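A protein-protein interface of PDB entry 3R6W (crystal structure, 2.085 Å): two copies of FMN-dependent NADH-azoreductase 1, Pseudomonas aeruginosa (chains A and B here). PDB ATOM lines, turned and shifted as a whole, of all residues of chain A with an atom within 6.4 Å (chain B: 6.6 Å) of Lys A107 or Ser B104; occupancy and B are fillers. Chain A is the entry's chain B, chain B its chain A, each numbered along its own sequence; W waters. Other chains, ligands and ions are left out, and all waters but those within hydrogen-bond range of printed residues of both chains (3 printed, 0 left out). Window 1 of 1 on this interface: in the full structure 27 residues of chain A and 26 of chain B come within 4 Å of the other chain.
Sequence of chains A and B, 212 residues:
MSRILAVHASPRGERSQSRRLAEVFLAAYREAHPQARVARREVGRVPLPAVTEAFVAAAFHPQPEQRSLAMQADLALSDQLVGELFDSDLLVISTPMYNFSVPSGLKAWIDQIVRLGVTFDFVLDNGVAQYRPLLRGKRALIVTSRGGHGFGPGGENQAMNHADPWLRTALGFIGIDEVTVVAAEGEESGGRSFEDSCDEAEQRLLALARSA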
ATOM      1  N   LEU A  48     -37.766 -25.636  19.392  1.00  0.00           N
ATOM      2  CA  LEU A  48     -37.484 -24.916  20.631  1.00  0.00           C
ATOM      3  C   LEU A  48     -36.080 -24.296  20.604  1.00  0.00           C
ATOM      4  O   LEU A  48     -35.098 -24.983  20.342  1.00  0.00           O
ATOM      5  CB  LEU A  48     -37.596 -25.869  21.812  1.00  0.00           C
ATOM      6  CG  LEU A  48     -38.495 -25.408  22.949  1.00  0.00           C
ATOM      7  CD1 LEU A  48     -39.957 -25.462  22.528  1.00  0.00           C
ATOM      8  CD2 LEU A  48     -38.254 -26.276  24.141  1.00  0.00           C
ATOM      9  N   PRO A  49     -35.979 -22.988  20.882  1.00  0.00           N
ATOM     10  CA  PRO A  49     -34.664 -22.333  20.877  1.00  0.00           C
ATOM     11  C   PRO A  49     -33.670 -22.878  21.914  1.00  0.00           C
ATOM     12  O   PRO A  49     -34.040 -23.240  23.038  1.00  0.00           O
ATOM     13  CB  PRO A  49     -34.995 -20.869  21.177  1.00  0.00           C
ATOM     14  CG  PRO A  49     -36.388 -20.870  21.696  1.00  0.00           C
ATOM     15  CD  PRO A  49     -37.075 -22.025  21.067  1.00  0.00           C
ATOM     16  N   ALA A  50     -32.404 -22.935  21.514  1.00  0.00           N
ATOM     17  CA  ALA A  50     -31.325 -23.316  22.414  1.00  0.00           C
ATOM     18  C   ALA A  50     -30.994 -22.166  23.359  1.00  0.00           C
ATOM     19  O   ALA A  50     -31.247 -21.005  23.053  1.00  0.00           O
ATOM     20  CB  ALA A  50     -30.090 -23.692  21.623  1.00  0.00           C
ATOM     21  N   VAL A  51     -30.414 -22.502  24.503  1.00  0.00           N
ATOM     22  CA  VAL A  51     -29.850 -21.502  25.390  1.00  0.00           C
ATOM     23  C   VAL A  51     -28.786 -20.698  24.637  1.00  0.00           C
ATOM     24  O   VAL A  51     -27.976 -21.271  23.900  1.00  0.00           O
ATOM     25  CB  VAL A  51     -29.245 -22.187  26.638  1.00  0.00           C
ATOM     26  CG1 VAL A  51     -28.219 -21.298  27.313  1.00  0.00           C
ATOM     27  CG2 VAL A  51     -30.355 -22.585  27.602  1.00  0.00           C
ATOM     28  N   SER A 101     -29.144 -40.806  23.265  1.00  0.00           N
ATOM     29  CA  SER A 101     -29.695 -39.759  24.115  1.00  0.00           C
ATOM     30  C   SER A 101     -31.105 -39.371  23.631  1.00  0.00           C
ATOM     31  O   SER A 101     -31.819 -40.211  23.090  1.00  0.00           O
ATOM     32  CB  SER A 101     -28.748 -38.553  24.145  1.00  0.00           C
ATOM     33  OG  SER A 101     -29.207 -37.551  25.032  1.00  0.00           O
ATOM     34  N   VAL A 102     -31.504 -38.115  23.844  1.00  0.00           N
ATOM     35  CA  VAL A 102     -32.838 -37.636  23.450  1.00  0.00           C
ATOM     36  C   VAL A 102     -32.730 -36.689  22.259  1.00  0.00           C
ATOM     37  O   VAL A 102     -31.672 -36.116  22.025  1.00  0.00           O
ATOM     38  CB  VAL A 102     -33.539 -36.868  24.595  1.00  0.00           C
ATOM     39  CG1 VAL A 102     -33.718 -37.751  25.835  1.00  0.00           C
ATOM     40  CG2 VAL A 102     -32.767 -35.603  24.938  1.00  0.00           C
ATOM     41  N   PRO A 103     -33.822 -36.516  21.500  1.00  0.00           N
ATOM     42  CA  PRO A 103     -33.762 -35.529  20.420  1.00  0.00           C
ATOM     43  C   PRO A 103     -33.351 -34.171  20.969  1.00  0.00           C
ATOM     44  O   PRO A 103     -33.632 -33.867  22.136  1.00  0.00           O
ATOM     45  CB  PRO A 103     -35.209 -35.479  19.914  1.00  0.00           C
ATOM     46  CG  PRO A 103     -35.766 -36.800  20.230  1.00  0.00           C
ATOM     47  CD  PRO A 103     -35.115 -37.226  21.526  1.00  0.00           C
ATOM     48  N   SER A 104     -32.689 -33.366  20.142  1.00  0.00           N
ATOM     49  CA  SER A 104     -32.117 -32.116  20.615  1.00  0.00           C
ATOM     50  C   SER A 104     -33.162 -31.123  21.161  1.00  0.00           C
ATOM     51  O   SER A 104     -32.856 -30.304  22.035  1.00  0.00           O
ATOM     52  CB  SER A 104     -31.266 -31.476  19.516  1.00  0.00           C
ATOM     53  OG  SER A 104     -32.053 -31.090  18.403  1.00  0.00           O
ATOM     54  N   GLY A 105     -34.385 -31.177  20.637  1.00  0.00           N
ATOM     55  CA  GLY A 105     -35.445 -30.303  21.113  1.00  0.00           C
ATOM     56  C   GLY A 105     -35.758 -30.565  22.584  1.00  0.00           C
ATOM     57  O   GLY A 105     -36.045 -29.644  23.349  1.00  0.00           O
ATOM     58  N   LEU A 106     -35.715 -31.831  22.990  1.00  0.00           N
ATOM     59  CA  LEU A 106     -35.966 -32.164  24.381  1.00  0.00           C
ATOM     60  C   LEU A 106     -34.805 -31.656  25.241  1.00  0.00           C
ATOM     61  O   LEU A 106     -35.025 -31.136  26.334  1.00  0.00           O
ATOM     62  CB  LEU A 106     -36.178 -33.671  24.563  1.00  0.00           C
ATOM     63  CG  LEU A 106     -36.466 -34.153  25.991  1.00  0.00           C
ATOM     64  CD1 LEU A 106     -37.500 -33.234  26.696  1.00  0.00           C
ATOM     65  CD2 LEU A 106     -36.926 -35.620  26.006  1.00  0.00           C
ATOM     66  N   LYS A 107     -33.568 -31.783  24.758  1.00  0.00           N
ATOM     67  CA  LYS A 107     -32.448 -31.214  25.519  1.00  0.00           C
ATOM     68  C   LYS A 107     -32.682 -29.714  25.705  1.00  0.00           C
ATOM     69  O   LYS A 107     -32.461 -29.156  26.790  1.00  0.00           O
ATOM     70  CB  LYS A 107     -31.102 -31.452  24.830  1.00  0.00           C
ATOM     71  CG  LYS A 107     -29.927 -30.870  25.636  1.00  0.00           C
ATOM     72  CD  LYS A 107     -29.655 -31.705  26.902  1.00  0.00           C
ATOM     73  CE  LYS A 107     -29.485 -30.804  28.123  1.00  0.00           C
ATOM     74  NZ  LYS A 107     -28.394 -29.772  27.975  1.00  0.00           N
ATOM     75  N   ALA A 108     -33.153 -29.061  24.644  1.00  0.00           N
ATOM     76  CA  ALA A 108     -33.427 -27.622  24.696  1.00  0.00           C
ATOM     77  C   ALA A 108     -34.518 -27.250  25.693  1.00  0.00           C
ATOM     78  O   ALA A 108     -34.429 -26.202  26.342  1.00  0.00           O
ATOM     79  CB  ALA A 108     -33.788 -27.089  23.315  1.00  0.00           C
ATOM     80  N   TRP A 109     -35.563 -28.082  25.783  1.00  0.00           N
ATOM     81  CA  TRP A 109     -36.632 -27.873  26.771  1.00  0.00           C
ATOM     82  C   TRP A 109     -36.038 -27.904  28.178  1.00  0.00           C
ATOM     83  O   TRP A 109     -36.208 -26.968  28.970  1.00  0.00           O
ATOM     84  CB  TRP A 109     -37.714 -28.960  26.662  1.00  0.00           C
ATOM     85  CG  TRP A 109     -38.844 -28.780  27.658  1.00  0.00           C
ATOM     86  CD1 TRP A 109     -39.844 -27.844  27.603  1.00  0.00           C
ATOM     87  CD2 TRP A 109     -39.089 -29.558  28.846  1.00  0.00           C
ATOM     88  NE1 TRP A 109     -40.685 -27.981  28.688  1.00  0.00           N
ATOM     89  CE2 TRP A 109     -40.248 -29.026  29.462  1.00  0.00           C
ATOM     90  CE3 TRP A 109     -38.439 -30.643  29.451  1.00  0.00           C
ATOM     91  CZ2 TRP A 109     -40.774 -29.546  30.650  1.00  0.00           C
ATOM     92  CZ3 TRP A 109     -38.965 -31.160  30.644  1.00  0.00           C
ATOM     93  CH2 TRP A 109     -40.123 -30.610  31.222  1.00  0.00           C
ATOM     94  N   ILE A 110     -35.332 -28.987  28.489  1.00  0.00           N
ATOM     95  CA  ILE A 110     -34.694 -29.088  29.794  1.00  0.00           C
ATOM     96  C   ILE A 110     -33.846 -27.844  30.069  1.00  0.00           C
ATOM     97  O   ILE A 110     -33.891 -27.280  31.166  1.00  0.00           O
ATOM     98  CB  ILE A 110     -33.804 -30.335  29.897  1.00  0.00           C
ATOM     99  CG1 ILE A 110     -34.661 -31.611  29.903  1.00  0.00           C
ATOM    100  CG2 ILE A 110     -32.944 -30.275  31.167  1.00  0.00           C
ATOM    101  CD1 ILE A 110     -35.443 -31.822  31.199  1.00  0.00           C
ATOM    102  N   ASP A 111     -33.079 -27.410  29.074  1.00  0.00           N
ATOM    103  CA  ASP A 111     -32.199 -26.252  29.269  1.00  0.00           C
ATOM    104  C   ASP A 111     -32.976 -24.960  29.556  1.00  0.00           C
ATOM    105  O   ASP A 111     -32.435 -24.017  30.124  1.00  0.00           O
ATOM    106  CB  ASP A 111     -31.234 -26.074  28.081  1.00  0.00           C
ATOM    107  CG  ASP A 111     -30.091 -27.089  28.095  1.00  0.00           C
ATOM    108  OD1 ASP A 111     -29.874 -27.721  29.152  1.00  0.00           O
ATOM    109  OD2 ASP A 111     -29.407 -27.251  27.055  1.00  0.00           O
ATOM    110  N   GLN A 112     -34.244 -24.910  29.152  1.00  0.00           N
ATOM    111  CA  GLN A 112     -35.063 -23.741  29.443  1.00  0.00           C
ATOM    112  C   GLN A 112     -35.666 -23.787  30.848  1.00  0.00           C
ATOM    113  O   GLN A 112     -35.901 -22.748  31.454  1.00  0.00           O
ATOM    114  CB  GLN A 112     -36.183 -23.560  28.395  1.00  0.00           C
ATOM    115  CG  GLN A 112     -35.693 -23.134  27.007  1.00  0.00           C
ATOM    116  CD  GLN A 112     -35.080 -21.722  26.982  1.00  0.00           C
ATOM    117  OE1 GLN A 112     -35.619 -20.786  27.571  1.00  0.00           O
ATOM    118  NE2 GLN A 112     -33.936 -21.578  26.303  1.00  0.00           N
ATOM    119  N   TRP A 166     -30.613 -40.067  31.827  1.00  0.00           N
ATOM    120  CA  TRP A 166     -30.194 -38.670  31.941  1.00  0.00           C
ATOM    121  C   TRP A 166     -31.355 -37.763  32.381  1.00  0.00           C
ATOM    122  O   TRP A 166     -31.174 -36.857  33.208  1.00  0.00           O
ATOM    123  CB  TRP A 166     -29.560 -38.118  30.658  1.00  0.00           C
ATOM    124  CG  TRP A 166     -29.556 -36.629  30.699  1.00  0.00           C
ATOM    125  CD1 TRP A 166     -28.743 -35.833  31.445  1.00  0.00           C
ATOM    126  CD2 TRP A 166     -30.469 -35.749  30.019  1.00  0.00           C
ATOM    127  NE1 TRP A 166     -29.068 -34.508  31.247  1.00  0.00           N
ATOM    128  CE2 TRP A 166     -30.121 -34.432  30.376  1.00  0.00           C
ATOM    129  CE3 TRP A 166     -31.525 -35.950  29.129  1.00  0.00           C
ATOM    130  CZ2 TRP A 166     -30.805 -33.320  29.888  1.00  0.00           C
ATOM    131  CZ3 TRP A 166     -32.197 -34.844  28.639  1.00  0.00           C
ATOM    132  CH2 TRP A 166     -31.837 -33.547  29.027  1.00  0.00           C
ATOM    133  N   ALA B   9     -19.233 -25.853  20.895  1.00  0.00           N
ATOM    134  CA  ALA B   9     -20.625 -26.017  21.287  1.00  0.00           C
ATOM    135  C   ALA B   9     -21.106 -25.046  22.378  1.00  0.00           C
ATOM    136  O   ALA B   9     -22.292 -25.028  22.707  1.00  0.00           O
ATOM    137  CB  ALA B   9     -20.905 -27.459  21.677  1.00  0.00           C
ATOM    138  N   VAL B  43     -21.510 -24.738  16.525  1.00  0.00           N
ATOM    139  CA  VAL B  43     -22.816 -25.308  16.876  1.00  0.00           C
ATOM    140  C   VAL B  43     -23.368 -24.699  18.178  1.00  0.00           C
ATOM    141  O   VAL B  43     -24.443 -25.078  18.647  1.00  0.00           O
ATOM    142  CB  VAL B  43     -22.796 -26.871  16.934  1.00  0.00           C
ATOM    143  CG1 VAL B  43     -22.211 -27.458  15.617  1.00  0.00           C
ATOM    144  CG2 VAL B  43     -22.013 -27.380  18.166  1.00  0.00           C
ATOM    145  N   LEU B  48     -28.250 -24.774  15.202  1.00  0.00           N
ATOM    146  CA  LEU B  48     -28.222 -25.896  14.264  1.00  0.00           C
ATOM    147  C   LEU B  48     -29.570 -26.635  14.248  1.00  0.00           C
ATOM    148  O   LEU B  48     -30.053 -27.080  15.281  1.00  0.00           O
ATOM    149  CB  LEU B  48     -27.096 -26.851  14.644  1.00  0.00           C
ATOM    150  CG  LEU B  48     -26.368 -27.608  13.537  1.00  0.00           C
ATOM    151  CD1 LEU B  48     -25.506 -26.669  12.718  1.00  0.00           C
ATOM    152  CD2 LEU B  48     -25.524 -28.690  14.152  1.00  0.00           C
ATOM    153  N   MET B  97     -20.725 -28.423  30.097  1.00  0.00           N
ATOM    154  CA  MET B  97     -21.743 -29.307  30.635  1.00  0.00           C
ATOM    155  C   MET B  97     -22.960 -28.448  30.940  1.00  0.00           C
ATOM    156  O   MET B  97     -22.880 -27.483  31.707  1.00  0.00           O
ATOM    157  CB  MET B  97     -21.276 -30.016  31.911  1.00  0.00           C
ATOM    158  CG  MET B  97     -22.434 -30.744  32.609  1.00  0.00           C
ATOM    159  SD  MET B  97     -21.961 -31.741  34.035  1.00  0.00           S
ATOM    160  CE  MET B  97     -21.387 -33.240  33.228  1.00  0.00           C
ATOM    161  N   TYR B  98     -24.079 -28.774  30.308  1.00  0.00           N
ATOM    162  CA  TYR B  98     -25.327 -28.043  30.518  1.00  0.00           C
ATOM    163  C   TYR B  98     -26.336 -29.045  31.034  1.00  0.00           C
ATOM    164  O   TYR B  98     -26.725 -29.955  30.302  1.00  0.00           O
ATOM    165  CB  TYR B  98     -25.882 -27.490  29.198  1.00  0.00           C
ATOM    166  CG  TYR B  98     -25.465 -26.090  28.844  1.00  0.00           C
ATOM    167  CD1 TYR B  98     -24.459 -25.441  29.548  1.00  0.00           C
ATOM    168  CD2 TYR B  98     -26.071 -25.419  27.785  1.00  0.00           C
ATOM    169  CE1 TYR B  98     -24.068 -24.149  29.216  1.00  0.00           C
ATOM    170  CE2 TYR B  98     -25.696 -24.120  27.448  1.00  0.00           C
ATOM    171  CZ  TYR B  98     -24.694 -23.497  28.169  1.00  0.00           C
ATOM    172  OH  TYR B  98     -24.310 -22.225  27.848  1.00  0.00           O
ATOM    173  N   ASN B  99     -26.757 -28.879  32.281  1.00  0.00           N
ATOM    174  CA  ASN B  99     -27.728 -29.781  32.882  1.00  0.00           C
ATOM    175  C   ASN B  99     -27.365 -31.257  32.722  1.00  0.00           C
ATOM    176  O   ASN B  99     -28.184 -32.078  32.312  1.00  0.00           O
ATOM    177  CB  ASN B  99     -29.131 -29.428  32.373  1.00  0.00           C
ATOM    178  CG  ASN B  99     -29.544 -28.031  32.816  1.00  0.00           C
ATOM    179  OD1 ASN B  99     -29.427 -27.697  34.006  1.00  0.00           O
ATOM    180  ND2 ASN B  99     -29.961 -27.194  31.870  1.00  0.00           N
ATOM    181  N   PHE B 100     -26.113 -31.569  33.066  1.00  0.00           N
ATOM    182  CA  PHE B 100     -25.626 -32.935  33.115  1.00  0.00           C
ATOM    183  C   PHE B 100     -25.501 -33.560  31.742  1.00  0.00           C
ATOM    184  O   PHE B 100     -25.217 -34.754  31.616  1.00  0.00           O
ATOM    185  CB  PHE B 100     -26.498 -33.765  34.047  1.00  0.00           C
ATOM    186  CG  PHE B 100     -26.692 -33.112  35.382  1.00  0.00           C
ATOM    187  CD1 PHE B 100     -25.676 -33.132  36.325  1.00  0.00           C
ATOM    188  CD2 PHE B 100     -27.864 -32.420  35.675  1.00  0.00           C
ATOM    189  CE1 PHE B 100     -25.831 -32.505  37.545  1.00  0.00           C
ATOM    190  CE2 PHE B 100     -28.025 -31.792  36.900  1.00  0.00           C
ATOM    191  CZ  PHE B 100     -27.006 -31.833  37.832  1.00  0.00           C
ATOM    192  N   SER B 101     -25.691 -32.744  30.712  1.00  0.00           N
ATOM    193  CA  SER B 101     -25.382 -33.184  29.363  1.00  0.00           C
ATOM    194  C   SER B 101     -24.709 -32.041  28.578  1.00  0.00           C
ATOM    195  O   SER B 101     -24.103 -31.147  29.175  1.00  0.00           O
ATOM    196  CB  SER B 101     -26.645 -33.703  28.679  1.00  0.00           C
ATOM    197  OG  SER B 101     -26.354 -34.321  27.435  1.00  0.00           O
ATOM    198  N   VAL B 102     -24.814 -32.081  27.251  1.00  0.00           N
ATOM    199  CA  VAL B 102     -24.225 -31.065  26.380  1.00  0.00           C
ATOM    200  C   VAL B 102     -25.322 -30.086  25.940  1.00  0.00           C
ATOM    201  O   VAL B 102     -26.507 -30.405  26.024  1.00  0.00           O
ATOM    202  CB  VAL B 102     -23.616 -31.705  25.099  1.00  0.00           C
ATOM    203  CG1 VAL B 102     -22.561 -32.742  25.455  1.00  0.00           C
ATOM    204  CG2 VAL B 102     -24.714 -32.347  24.278  1.00  0.00           C
ATOM    205  N   PRO B 103     -24.929 -28.891  25.459  1.00  0.00           N
ATOM    206  CA  PRO B 103     -25.914 -27.969  24.899  1.00  0.00           C
ATOM    207  C   PRO B 103     -26.666 -28.599  23.736  1.00  0.00           C
ATOM    208  O   PRO B 103     -26.120 -29.439  23.005  1.00  0.00           O
ATOM    209  CB  PRO B 103     -25.054 -26.799  24.405  1.00  0.00           C
ATOM    210  CG  PRO B 103     -23.824 -26.863  25.261  1.00  0.00           C
ATOM    211  CD  PRO B 103     -23.568 -28.333  25.394  1.00  0.00           C
ATOM    212  N   SER B 104     -27.921 -28.189  23.567  1.00  0.00           N
ATOM    213  CA  SER B 104     -28.792 -28.853  22.615  1.00  0.00           C
ATOM    214  C   SER B 104     -28.232 -28.771  21.183  1.00  0.00           C
ATOM    215  O   SER B 104     -28.376 -29.717  20.400  1.00  0.00           O
ATOM    216  CB  SER B 104     -30.205 -28.282  22.709  1.00  0.00           C
ATOM    217  OG  SER B 104     -30.208 -26.977  22.202  1.00  0.00           O
ATOM    218  N   GLY B 105     -27.560 -27.668  20.849  1.00  0.00           N
ATOM    219  CA  GLY B 105     -26.940 -27.532  19.535  1.00  0.00           C
ATOM    220  C   GLY B 105     -25.926 -28.629  19.210  1.00  0.00           C
ATOM    221  O   GLY B 105     -25.789 -29.066  18.052  1.00  0.00           O
ATOM    222  N   LEU B 106     -25.207 -29.091  20.232  1.00  0.00           N
ATOM    223  CA  LEU B 106     -24.221 -30.149  20.023  1.00  0.00           C
ATOM    224  C   LEU B 106     -24.939 -31.467  19.797  1.00  0.00           C
ATOM    225  O   LEU B 106     -24.506 -32.298  18.985  1.00  0.00           O
ATOM    226  CB  LEU B 106     -23.266 -30.276  21.232  1.00  0.00           C
ATOM    227  CG  LEU B 106     -22.183 -31.360  21.098  1.00  0.00           C
ATOM    228  CD1 LEU B 106     -21.504 -31.291  19.725  1.00  0.00           C
ATOM    229  CD2 LEU B 106     -21.128 -31.286  22.234  1.00  0.00           C
ATOM    230  N   LYS B 107     -26.021 -31.669  20.538  1.00  0.00           N
ATOM    231  CA  LYS B 107     -26.840 -32.857  20.346  1.00  0.00           C
ATOM    232  C   LYS B 107     -27.374 -32.845  18.911  1.00  0.00           C
ATOM    233  O   LYS B 107     -27.385 -33.878  18.230  1.00  0.00           O
ATOM    234  CB  LYS B 107     -27.988 -32.904  21.371  1.00  0.00           C
ATOM    235  CG  LYS B 107     -28.883 -34.128  21.237  1.00  0.00           C
ATOM    236  CD  LYS B 107     -28.194 -35.388  21.724  1.00  0.00           C
ATOM    237  CE  LYS B 107     -28.344 -36.564  20.740  1.00  0.00           C
ATOM    238  NZ  LYS B 107     -29.753 -36.901  20.375  1.00  0.00           N
ATOM    239  N   ALA B 108     -27.803 -31.676  18.437  1.00  0.00           N
ATOM    240  CA  ALA B 108     -28.334 -31.604  17.076  1.00  0.00           C
ATOM    241  C   ALA B 108     -27.239 -31.919  16.047  1.00  0.00           C
ATOM    242  O   ALA B 108     -27.499 -32.565  15.035  1.00  0.00           O
ATOM    243  CB  ALA B 108     -28.985 -30.259  16.798  1.00  0.00           C
ATOM    244  N   TRP B 109     -26.013 -31.482  16.315  1.00  0.00           N
ATOM    245  CA  TRP B 109     -24.900 -31.770  15.404  1.00  0.00           C
ATOM    246  C   TRP B 109     -24.704 -33.272  15.286  1.00  0.00           C
ATOM    247  O   TRP B 109     -24.589 -33.825  14.177  1.00  0.00           O
ATOM    248  CB  TRP B 109     -23.602 -31.113  15.878  1.00  0.00           C
ATOM    249  CG  TRP B 109     -22.445 -31.404  14.962  1.00  0.00           C
ATOM    250  CD1 TRP B 109     -22.205 -30.835  13.759  1.00  0.00           C
ATOM    251  CD2 TRP B 109     -21.378 -32.329  15.187  1.00  0.00           C
ATOM    252  NE1 TRP B 109     -21.060 -31.346  13.207  1.00  0.00           N
ATOM    253  CE2 TRP B 109     -20.528 -32.264  14.065  1.00  0.00           C
ATOM    254  CE3 TRP B 109     -21.063 -33.210  16.221  1.00  0.00           C
ATOM    255  CZ2 TRP B 109     -19.373 -33.048  13.947  1.00  0.00           C
ATOM    256  CZ3 TRP B 109     -19.915 -33.995  16.105  1.00  0.00           C
ATOM    257  CH2 TRP B 109     -19.087 -33.905  14.979  1.00  0.00           C
HETATM  258  O   HOH W   1     -30.782 -24.394  32.166  1.00  0.00           O
HETATM  259  O   HOH W   2     -27.302 -36.916  27.119  1.00  0.00           O
HETATM  260  O   HOH W   3     -29.421 -25.658  25.009  1.00  0.00           O
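The backbone carbonyl oxygen (O) of Tyr B98 lies within hydrogen-bond range of the side-chain amino group (NZ) of Lys A107 (2.9 Å).
The side-chain amino group of Lys B107 is in hydrogen-bond range of the backbone carbonyl oxygen of Val A102, at 2.6 Å.
The side-chain carboxylate (OD1) of Asp A111 sits at hydrogen-bond distance from the side-chain amide nitrogen (ND2) of Asn B99, 2.8 Å away.
The indole nitrogen (NE1) of Trp A166 is in hydrogen-bond range of the backbone carbonyl oxygen (O) of Asn B99 (2.8 Å).
NZ of Lys A107 is in hydrogen-bond range of O of Val B102 (2.8 Å).
NZ of Lys A107 lies within salt-bridge range of OD1 of Asp A111.
OG of Ser B104 touches CB of Ala A50 (3.3 Å).
Tyr B98 touches Val A51.
Lys B107 touches Ser A101.
O of Ser A104 touches CB of Ser B104, at 3.4 Å.
Lys B107 touches Ser A104 (CG to CA, 3.9 Å).
Ile A110 touches Asn B99 (O to ND2, 3.99 Å).
OD2 of Asp A111 touches CD2 of Tyr B98 (3.9 Å).
Asp A111 touches Ser B104 (OD2 to N, 3.9 Å).
Trp A166 touches Phe B100.
Trp A166 touches Ser B101 (NE1 to CB, 3.6 Å).
Lys A107 touches just these residues of chain B: Tyr B98 (2.9 Å), Val B102 (2.8 Å) and Ser B104 (3.8 Å).
Ser B104 touches five residues of chain A.
Printed residues of chain A within 4 Å of Val B102: Lys A107.
Of the printed residues of chain A, Phe B100 touches Trp A166 (3.7 Å).
Printed residues of chain B within 4 Å of Ala A108: Ser B104.
Gln A112 touches none of the printed residues of chain B.
Pro A49 touches none of the printed residues of chain B.
The nearest residue of chain B that does not touch Lys A107 is Ser B101 (4.03 Å).
The nearest residue of chain A that does not touch Ser B104 is Val A51 (5.0 Å).
The nearest printed residue of chain B that does not touch Asp A111 is Pro B103 (4.2 Å).
Of the 17 printed residues of chain A, 10 touch a printed residue of chain B.
Printed residues of chain A that touch a printed residue of chain B: Ala A50, Val A51, Ser A101, Val A102, Ser A104, Lys A107, Ala A108, Ile A110, Asp A111 and Trp A166.
Hydrophobic or aromatic side chains of chain B within 4 Å of the printed part of chain A: Tyr B98, Phe B100 and Ala B108.
Among the printed residues, no Asp or Glu carboxylate lies within 4 Å of a Lys or Arg side-chain nitrogen of the other chain.
Ser A101 touches Lys B107, but with the chains exchanged Lys A107 does not touch Ser B101 (4.03 Å).
Val A102 touches Lys B107, and with the chains exchanged Lys A107 touches Val B102.
Ser A104 touches its own counterpart, Ser B104.
Ser A104 touches Lys B107, and with the chains exchanged Lys A107 touches Ser B104.
Of the 18 pairs that touch across the chains among the printed residues, 7 have their exchanged pair printed and touching as well.
Water W3 lies within hydrogen-bond range of the side-chain carboxylate (OD2) of Asp A111 (2.6 Å), the side-chain hydroxyl (OG) of Ser B104 (3.2 Å) and the backbone NH (N) of Val A51 (3.3 Å).
Water W1 bridges the backbone carbonyl oxygen (O) of Asp A111 (2.7 Å) and the side-chain amide nitrogen (ND2) of Asn B99 (2.9 Å).
Water W2 lies within hydrogen-bond range of the side-chain hydroxyl of Ser B101 (2.8 Å) and the side-chain hydroxyl of Ser A101 (2.9 Å).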
